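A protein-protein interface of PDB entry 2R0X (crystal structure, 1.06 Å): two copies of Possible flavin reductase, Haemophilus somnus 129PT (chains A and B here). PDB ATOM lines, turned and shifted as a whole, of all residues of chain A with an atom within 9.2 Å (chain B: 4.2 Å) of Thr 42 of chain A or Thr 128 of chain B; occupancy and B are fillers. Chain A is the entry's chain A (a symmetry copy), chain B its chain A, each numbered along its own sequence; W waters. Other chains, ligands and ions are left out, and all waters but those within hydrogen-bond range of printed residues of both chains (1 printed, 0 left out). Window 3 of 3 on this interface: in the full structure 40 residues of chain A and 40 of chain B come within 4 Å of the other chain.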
ATOM      1  N   CYS A  39      -1.771 -23.617  21.190  1.00  0.00           N
ATOM      2  CA  CYS A  39      -2.249 -23.338  19.852  1.00  0.00           C
ATOM      3  C   CYS A  39      -3.667 -23.833  19.725  1.00  0.00           C
ATOM      4  O   CYS A  39      -4.113 -24.684  20.507  1.00  0.00           O
ATOM      5  CB  CYS A  39      -1.334 -23.972  18.776  1.00  0.00           C
ATOM      6  SG  CYS A  39      -1.390 -25.787  18.761  1.00  0.00           S
ATOM      7  N   SER A  40      -4.385 -23.303  18.748  1.00  0.00           N
ATOM      8  CA  SER A  40      -5.669 -23.864  18.403  1.00  0.00           C
ATOM      9  C   SER A  40      -5.483 -25.221  17.759  1.00  0.00           C
ATOM     10  O   SER A  40      -4.439 -25.543  17.192  1.00  0.00           O
ATOM     11  CB  SER A  40      -6.450 -22.949  17.463  1.00  0.00           C
ATOM     12  OG  SER A  40      -5.762 -22.793  16.245  1.00  0.00           O
ATOM     13  N   VAL A  41      -6.540 -26.006  17.849  1.00  0.00           N
ATOM     14  CA  VAL A  41      -6.559 -27.354  17.337  1.00  0.00           C
ATOM     15  C   VAL A  41      -7.657 -27.471  16.323  1.00  0.00           C
ATOM     16  O   VAL A  41      -7.432 -27.810  15.156  1.00  0.00           O
ATOM     17  CB  VAL A  41      -6.833 -28.340  18.438  1.00  0.00           C
ATOM     18  CG1 VAL A  41      -7.008 -29.758  17.860  1.00  0.00           C
ATOM     19  CG2 VAL A  41      -5.692 -28.276  19.446  1.00  0.00           C
ATOM     20  N   THR A  42      -8.866 -27.185  16.778  1.00  0.00           N
ATOM     21  CA  THR A  42     -10.032 -27.364  15.929  1.00  0.00           C
ATOM     22  C   THR A  42     -11.108 -26.340  16.267  1.00  0.00           C
ATOM     23  O   THR A  42     -11.080 -25.750  17.357  1.00  0.00           O
ATOM     24  CB  THR A  42     -10.577 -28.838  16.040  1.00  0.00           C
ATOM     25  OG1 THR A  42     -11.611 -29.009  15.097  1.00  0.00           O
ATOM     26  CG2 THR A  42     -11.074 -29.146  17.448  1.00  0.00           C
ATOM     27  N   ASP A  43     -12.061 -26.167  15.372  1.00  0.00           N
ATOM     28  CA  ASP A  43     -13.222 -25.317  15.611  1.00  0.00           C
ATOM     29  C   ASP A  43     -14.511 -26.136  15.669  1.00  0.00           C
ATOM     30  O   ASP A  43     -15.617 -25.575  15.558  1.00  0.00           O
ATOM     31  CB  ASP A  43     -13.303 -24.246  14.521  1.00  0.00           C
ATOM     32  CG  ASP A  43     -13.448 -24.838  13.118  1.00  0.00           C
ATOM     33  OD1 ASP A  43     -13.163 -26.036  12.944  1.00  0.00           O
ATOM     34  OD2 ASP A  43     -13.835 -24.092  12.193  1.00  0.00           O
ATOM     35  N   SER A  44     -14.373 -27.437  15.929  1.00  0.00           N
ATOM     36  CA  SER A  44     -15.511 -28.348  15.995  1.00  0.00           C
ATOM     37  C   SER A  44     -15.377 -29.330  17.149  1.00  0.00           C
ATOM     38  O   SER A  44     -14.914 -30.470  16.985  1.00  0.00           O
ATOM     39  CB  SER A  44     -15.603 -29.105  14.683  1.00  0.00           C
ATOM     40  OG  SER A  44     -15.809 -28.194  13.612  1.00  0.00           O
ATOM     41  N   PRO A  45     -15.688 -28.886  18.347  1.00  0.00           N
ATOM     42  CA  PRO A  45     -15.955 -27.511  18.758  1.00  0.00           C
ATOM     43  C   PRO A  45     -14.633 -26.782  18.978  1.00  0.00           C
ATOM     44  O   PRO A  45     -13.601 -27.389  18.970  1.00  0.00           O
ATOM     45  CB  PRO A  45     -16.669 -27.718  20.076  1.00  0.00           C
ATOM     46  CG  PRO A  45     -16.009 -28.901  20.653  1.00  0.00           C
ATOM     47  CD  PRO A  45     -15.678 -29.779  19.513  1.00  0.00           C
ATOM     48  N   PRO A  46     -14.690 -25.460  19.179  1.00  0.00           N
ATOM     49  CA  PRO A  46     -13.484 -24.719  19.473  1.00  0.00           C
ATOM     50  C   PRO A  46     -12.678 -25.353  20.598  1.00  0.00           C
ATOM     51  O   PRO A  46     -13.177 -25.585  21.703  1.00  0.00           O
ATOM     52  CB  PRO A  46     -14.022 -23.331  19.839  1.00  0.00           C
ATOM     53  CG  PRO A  46     -15.206 -23.184  18.957  1.00  0.00           C
ATOM     54  CD  PRO A  46     -15.852 -24.550  19.042  1.00  0.00           C
ATOM     55  N   THR A  47     -11.431 -25.642  20.281  1.00  0.00           N
ATOM     56  CA  THR A  47     -10.532 -26.384  21.118  1.00  0.00           C
ATOM     57  C   THR A  47      -9.106 -25.868  20.964  1.00  0.00           C
ATOM     58  O   THR A  47      -8.654 -25.628  19.840  1.00  0.00           O
ATOM     59  CB  THR A  47     -10.541 -27.888  20.726  1.00  0.00           C
ATOM     60  OG1 THR A  47     -11.867 -28.380  20.827  1.00  0.00           O
ATOM     61  CG2 THR A  47      -9.682 -28.785  21.657  1.00  0.00           C
ATOM     62  N   LEU A  48      -8.363 -25.839  22.045  1.00  0.00           N
ATOM     63  CA  LEU A  48      -6.971 -25.485  21.964  1.00  0.00           C
ATOM     64  C   LEU A  48      -6.226 -26.560  22.732  1.00  0.00           C
ATOM     65  O   LEU A  48      -6.816 -27.380  23.444  1.00  0.00           O
ATOM     66  CB  LEU A  48      -6.784 -24.057  22.496  1.00  0.00           C
ATOM     67  CG  LEU A  48      -7.183 -23.759  23.942  1.00  0.00           C
ATOM     68  CD1 LEU A  48      -6.176 -24.320  24.903  1.00  0.00           C
ATOM     69  CD2 LEU A  48      -7.362 -22.275  24.171  1.00  0.00           C
ATOM     70  N   LEU A  49      -4.910 -26.544  22.561  1.00  0.00           N
ATOM     71  CA  LEU A  49      -4.048 -27.352  23.399  1.00  0.00           C
ATOM     72  C   LEU A  49      -3.039 -26.511  24.101  1.00  0.00           C
ATOM     73  O   LEU A  49      -2.697 -25.407  23.665  1.00  0.00           O
ATOM     74  CB  LEU A  49      -3.359 -28.463  22.595  1.00  0.00           C
ATOM     75  CG  LEU A  49      -2.339 -28.049  21.513  1.00  0.00           C
ATOM     76  CD1 LEU A  49      -0.978 -27.708  22.097  1.00  0.00           C
ATOM     77  CD2 LEU A  49      -2.139 -29.162  20.419  1.00  0.00           C
ATOM     78  N   ILE A 133      -5.703 -31.227  26.051  1.00  0.00           N
ATOM     79  CA  ILE A 133      -6.693 -30.931  25.025  1.00  0.00           C
ATOM     80  C   ILE A 133      -7.835 -30.222  25.694  1.00  0.00           C
ATOM     81  O   ILE A 133      -8.414 -30.758  26.647  1.00  0.00           O
ATOM     82  CB  ILE A 133      -7.246 -32.205  24.372  1.00  0.00           C
ATOM     83  CG1 ILE A 133      -6.130 -32.964  23.684  1.00  0.00           C
ATOM     84  CG2 ILE A 133      -8.302 -31.878  23.377  1.00  0.00           C
ATOM     85  CD1 ILE A 133      -5.341 -32.146  22.728  1.00  0.00           C
ATOM     86  N   CYS A 134      -8.148 -29.028  25.212  1.00  0.00           N
ATOM     87  CA  CYS A 134      -8.996 -28.120  25.988  1.00  0.00           C
ATOM     88  C   CYS A 134     -10.158 -27.580  25.165  1.00  0.00           C
ATOM     89  O   CYS A 134      -9.977 -26.715  24.318  1.00  0.00           O
ATOM     90  CB  CYS A 134      -8.133 -26.948  26.461  1.00  0.00           C
ATOM     91  SG  CYS A 134      -6.777 -27.417  27.554  1.00  0.00           S
ATOM     92  N   LYS A 135     -11.357 -28.024  25.505  1.00  0.00           N
ATOM     93  CA  LYS A 135     -12.560 -27.511  24.895  1.00  0.00           C
ATOM     94  C   LYS A 135     -12.826 -26.123  25.477  1.00  0.00           C
ATOM     95  O   LYS A 135     -12.905 -25.960  26.689  1.00  0.00           O
ATOM     96  CB  LYS A 135     -13.740 -28.433  25.193  1.00  0.00           C
ATOM     97  CG  LYS A 135     -15.022 -27.932  24.607  1.00  0.00           C
ATOM     98  CD  LYS A 135     -16.234 -28.788  25.076  1.00  0.00           C
ATOM     99  CE  LYS A 135     -17.507 -28.206  24.635  1.00  0.00           C
ATOM    100  NZ  LYS A 135     -18.585 -29.122  25.142  1.00  0.00           N
ATOM    101  N   ILE A 136     -13.035 -25.147  24.624  1.00  0.00           N
ATOM    102  CA  ILE A 136     -13.293 -23.761  25.053  1.00  0.00           C
ATOM    103  C   ILE A 136     -14.762 -23.606  25.407  1.00  0.00           C
ATOM    104  O   ILE A 136     -15.637 -23.914  24.610  1.00  0.00           O
ATOM    105  CB  ILE A 136     -12.886 -22.740  23.977  1.00  0.00           C
ATOM    106  CG1 ILE A 136     -11.378 -22.901  23.674  1.00  0.00           C
ATOM    107  CG2 ILE A 136     -13.232 -21.337  24.403  1.00  0.00           C
ATOM    108  CD1 ILE A 136     -11.012 -22.311  22.355  1.00  0.00           C
ATOM    109  N   PHE B   8     -14.878 -17.696  18.383  1.00  0.00           N
ATOM    110  CA  PHE B   8     -13.584 -18.323  18.510  1.00  0.00           C
ATOM    111  C   PHE B   8     -12.629 -17.850  17.427  1.00  0.00           C
ATOM    112  O   PHE B   8     -11.476 -17.540  17.735  1.00  0.00           O
ATOM    113  CB  PHE B   8     -13.752 -19.826  18.376  1.00  0.00           C
ATOM    114  CG  PHE B   8     -12.471 -20.608  18.384  1.00  0.00           C
ATOM    115  CD1 PHE B   8     -11.594 -20.496  19.434  1.00  0.00           C
ATOM    116  CD2 PHE B   8     -12.152 -21.467  17.355  1.00  0.00           C
ATOM    117  CE1 PHE B   8     -10.423 -21.241  19.476  1.00  0.00           C
ATOM    118  CE2 PHE B   8     -10.967 -22.209  17.406  1.00  0.00           C
ATOM    119  CZ  PHE B   8     -10.117 -22.089  18.451  1.00  0.00           C
ATOM    120  N   ASN B  53      -5.576 -30.540   9.423  1.00  0.00           N
ATOM    121  CA  ASN B  53      -6.954 -30.868   9.123  1.00  0.00           C
ATOM    122  C   ASN B  53      -6.981 -32.240   8.452  1.00  0.00           C
ATOM    123  O   ASN B  53      -6.374 -32.428   7.396  1.00  0.00           O
ATOM    124  CB  ASN B  53      -7.616 -29.790   8.243  1.00  0.00           C
ATOM    125  CG  ASN B  53      -9.127 -29.990   8.140  1.00  0.00           C
ATOM    126  OD1 ASN B  53      -9.594 -31.075   7.865  1.00  0.00           O
ATOM    127  ND2 ASN B  53      -9.888 -28.917   8.376  1.00  0.00           N
ATOM    128  N   SER B  54      -7.666 -33.200   9.061  1.00  0.00           N
ATOM    129  CA  SER B  54      -7.655 -34.561   8.535  1.00  0.00           C
ATOM    130  C   SER B  54      -8.479 -34.747   7.279  1.00  0.00           C
ATOM    131  O   SER B  54      -8.461 -35.810   6.681  1.00  0.00           O
ATOM    132  CB  SER B  54      -8.026 -35.592   9.569  1.00  0.00           C
ATOM    133  OG  SER B  54      -9.326 -35.361   9.986  1.00  0.00           O
ATOM    134  N   ASN B  55      -9.147 -33.691   6.858  1.00  0.00           N
ATOM    135  CA  ASN B  55      -9.902 -33.678   5.629  1.00  0.00           C
ATOM    136  C   ASN B  55      -9.177 -32.958   4.507  1.00  0.00           C
ATOM    137  O   ASN B  55      -9.693 -32.902   3.391  1.00  0.00           O
ATOM    138  CB  ASN B  55     -11.257 -33.004   5.869  1.00  0.00           C
ATOM    139  CG  ASN B  55     -11.990 -33.614   7.044  1.00  0.00           C
ATOM    140  OD1 ASN B  55     -12.500 -34.716   6.906  1.00  0.00           O
ATOM    141  ND2 ASN B  55     -11.961 -32.945   8.241  1.00  0.00           N
ATOM    142  N   VAL B 126      -8.274 -35.532  16.923  1.00  0.00           N
ATOM    143  CA  VAL B 126      -9.077 -34.567  17.644  1.00  0.00           C
ATOM    144  C   VAL B 126     -10.163 -34.022  16.710  1.00  0.00           C
ATOM    145  O   VAL B 126     -10.103 -32.891  16.214  1.00  0.00           O
ATOM    146  CB  VAL B 126      -8.221 -33.410  18.218  1.00  0.00           C
ATOM    147  CG1 VAL B 126      -9.072 -32.513  19.186  1.00  0.00           C
ATOM    148  CG2 VAL B 126      -7.023 -33.968  18.982  1.00  0.00           C
ATOM    149  N   GLY B 127     -11.135 -34.881  16.421  1.00  0.00           N
ATOM    150  CA  GLY B 127     -12.218 -34.508  15.535  1.00  0.00           C
ATOM    151  C   GLY B 127     -11.784 -34.257  14.096  1.00  0.00           C
ATOM    152  O   GLY B 127     -11.269 -35.148  13.446  1.00  0.00           O
ATOM    153  N   THR B 128     -12.043 -33.050  13.601  1.00  0.00           N
ATOM    154  CA  THR B 128     -11.678 -32.708  12.228  1.00  0.00           C
ATOM    155  C   THR B 128     -10.162 -32.533  12.041  1.00  0.00           C
ATOM    156  O   THR B 128      -9.717 -32.419  10.905  1.00  0.00           O
ATOM    157  CB  THR B 128     -12.347 -31.428  11.762  1.00  0.00           C
ATOM    158  OG1 THR B 128     -11.958 -30.381  12.637  1.00  0.00           O
ATOM    159  CG2 THR B 128     -13.865 -31.587  11.730  1.00  0.00           C
ATOM    160  N   HIS B 129      -9.404 -32.464  13.129  1.00  0.00           N
ATOM    161  CA  HIS B 129      -7.961 -32.303  13.040  1.00  0.00           C
ATOM    162  C   HIS B 129      -7.271 -33.459  13.724  1.00  0.00           C
ATOM    163  O   HIS B 129      -7.818 -34.137  14.611  1.00  0.00           O
ATOM    164  CB  HIS B 129      -7.510 -30.957  13.660  1.00  0.00           C
ATOM    165  CG  HIS B 129      -7.898 -29.789  12.844  1.00  0.00           C
ATOM    166  ND1 HIS B 129      -9.205 -29.418  12.630  1.00  0.00           N
ATOM    167  CD2 HIS B 129      -7.140 -28.891  12.189  1.00  0.00           C
ATOM    168  CE1 HIS B 129      -9.230 -28.324  11.876  1.00  0.00           C
ATOM    169  NE2 HIS B 129      -7.991 -28.012  11.565  1.00  0.00           N
HETATM  170  O   HOH W   1     -12.940 -31.263  15.659  1.00  0.00           O
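The side-chain hydroxyl (OG1) of Thr 42 of chain A is in hydrogen-bond range of the side-chain hydroxyl (OG1) of Thr 128 of chain B (2.8 Å).
A ring nitrogen (ND1) of His 129 of chain B sits close to the backbone carbonyl oxygen of Val 41 of chain A, at 3.5 Å.
ND1 of His 129 of chain B sits at hydrogen-bond distance from OG1 of Thr 42 of chain A, at 3.5 Å.
The backbone carbonyl oxygen of Thr 128 of chain B lies close to the side-chain amide oxygen of Asn 53 of chain B.
The backbone carbonyl oxygen (O) of Thr 128 of chain B is in hydrogen-bond range of the backbone NH (N) of Ser 54 of chain B.
The side-chain hydroxyl (OG1) of Thr 128 of chain B sits at hydrogen-bond distance from a ring nitrogen (ND1) of His 129 of chain B (2.9 Å).
N of Val 41 of chain A is in hydrogen-bond range of O of Thr 47 of chain A, at 2.9 Å.
The backbone carbonyl oxygen of Thr 42 of chain A is in hydrogen-bond range of the backbone NH of Thr 47 of chain A, 2.9 Å away.
N of Ile 136 of chain A lies within hydrogen-bond range of O of Pro 46 of chain A.
CZ of Phe 8 of chain B touches CB of Ser 40 of chain A, at 3.9 Å.
Val 126 of chain B touches Val 41 of chain A.
O of Thr 42 of chain A touches CE2 of Phe 8 of chain B (3.5 Å).
Phe 8 of chain B touches Pro 46 of chain A (CG to CB, 3.5 Å).
Phe 8 of chain B touches Ile 136 of chain A.
Thr 42 of chain A touches just these residues of chain B: Phe 8 (3.5 Å), Thr 128 (2.8 Å) and His 129 (3.5 Å).
Printed residues of chain A within 4 Å of Thr 128 of chain B: Thr 42 (2.8 Å).
No residue of chain A comes within 4 Å of Asn 53 of chain B.
Of the printed residues of chain B, Ser 40 of chain A touches Phe 8 (3.9 Å).
Printed residues of chain A within 4 Å of His 129 of chain B: Val 41 and Thr 42.
Of the printed residues of chain B, Val 41 of chain A touches Val 126 and His 129.
Thr 47 of chain A touches none of the printed residues of chain B.
The nearest residue of chain B that does not touch Thr 42 of chain A is Val 126 of chain B (4.1 Å).
The nearest printed residue of chain A that does not touch Thr 128 of chain B is Ser 44 of chain A (4.2 Å).
Of the 15 printed residues of chain A, 5 touch a printed residue of chain B.
Hydrophobic or aromatic side chains of chain A that line the printed part of chain B: Val 41, Pro 46 and Ile 136.
Among the printed residues, no Asp or Glu carboxylate lies within 4 Å of a Lys or Arg side-chain nitrogen of the other chain.
No position is printed for both chains.
Of the 8 pairs that touch across the chains among the printed residues, none has its exchanged pair printed and touching as well.
Water W1 lies within hydrogen-bond range of the backbone carbonyl oxygen (O) of Ser 44 of chain A (2.5 Å), the side-chain hydroxyl (OG1) of Thr 42 of chain A (2.7 Å), the backbone NH (N) of Thr 128 of chain B (2.9 Å) and the backbone carbonyl oxygen (O) of Val 126 of chain B (3.3 Å).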
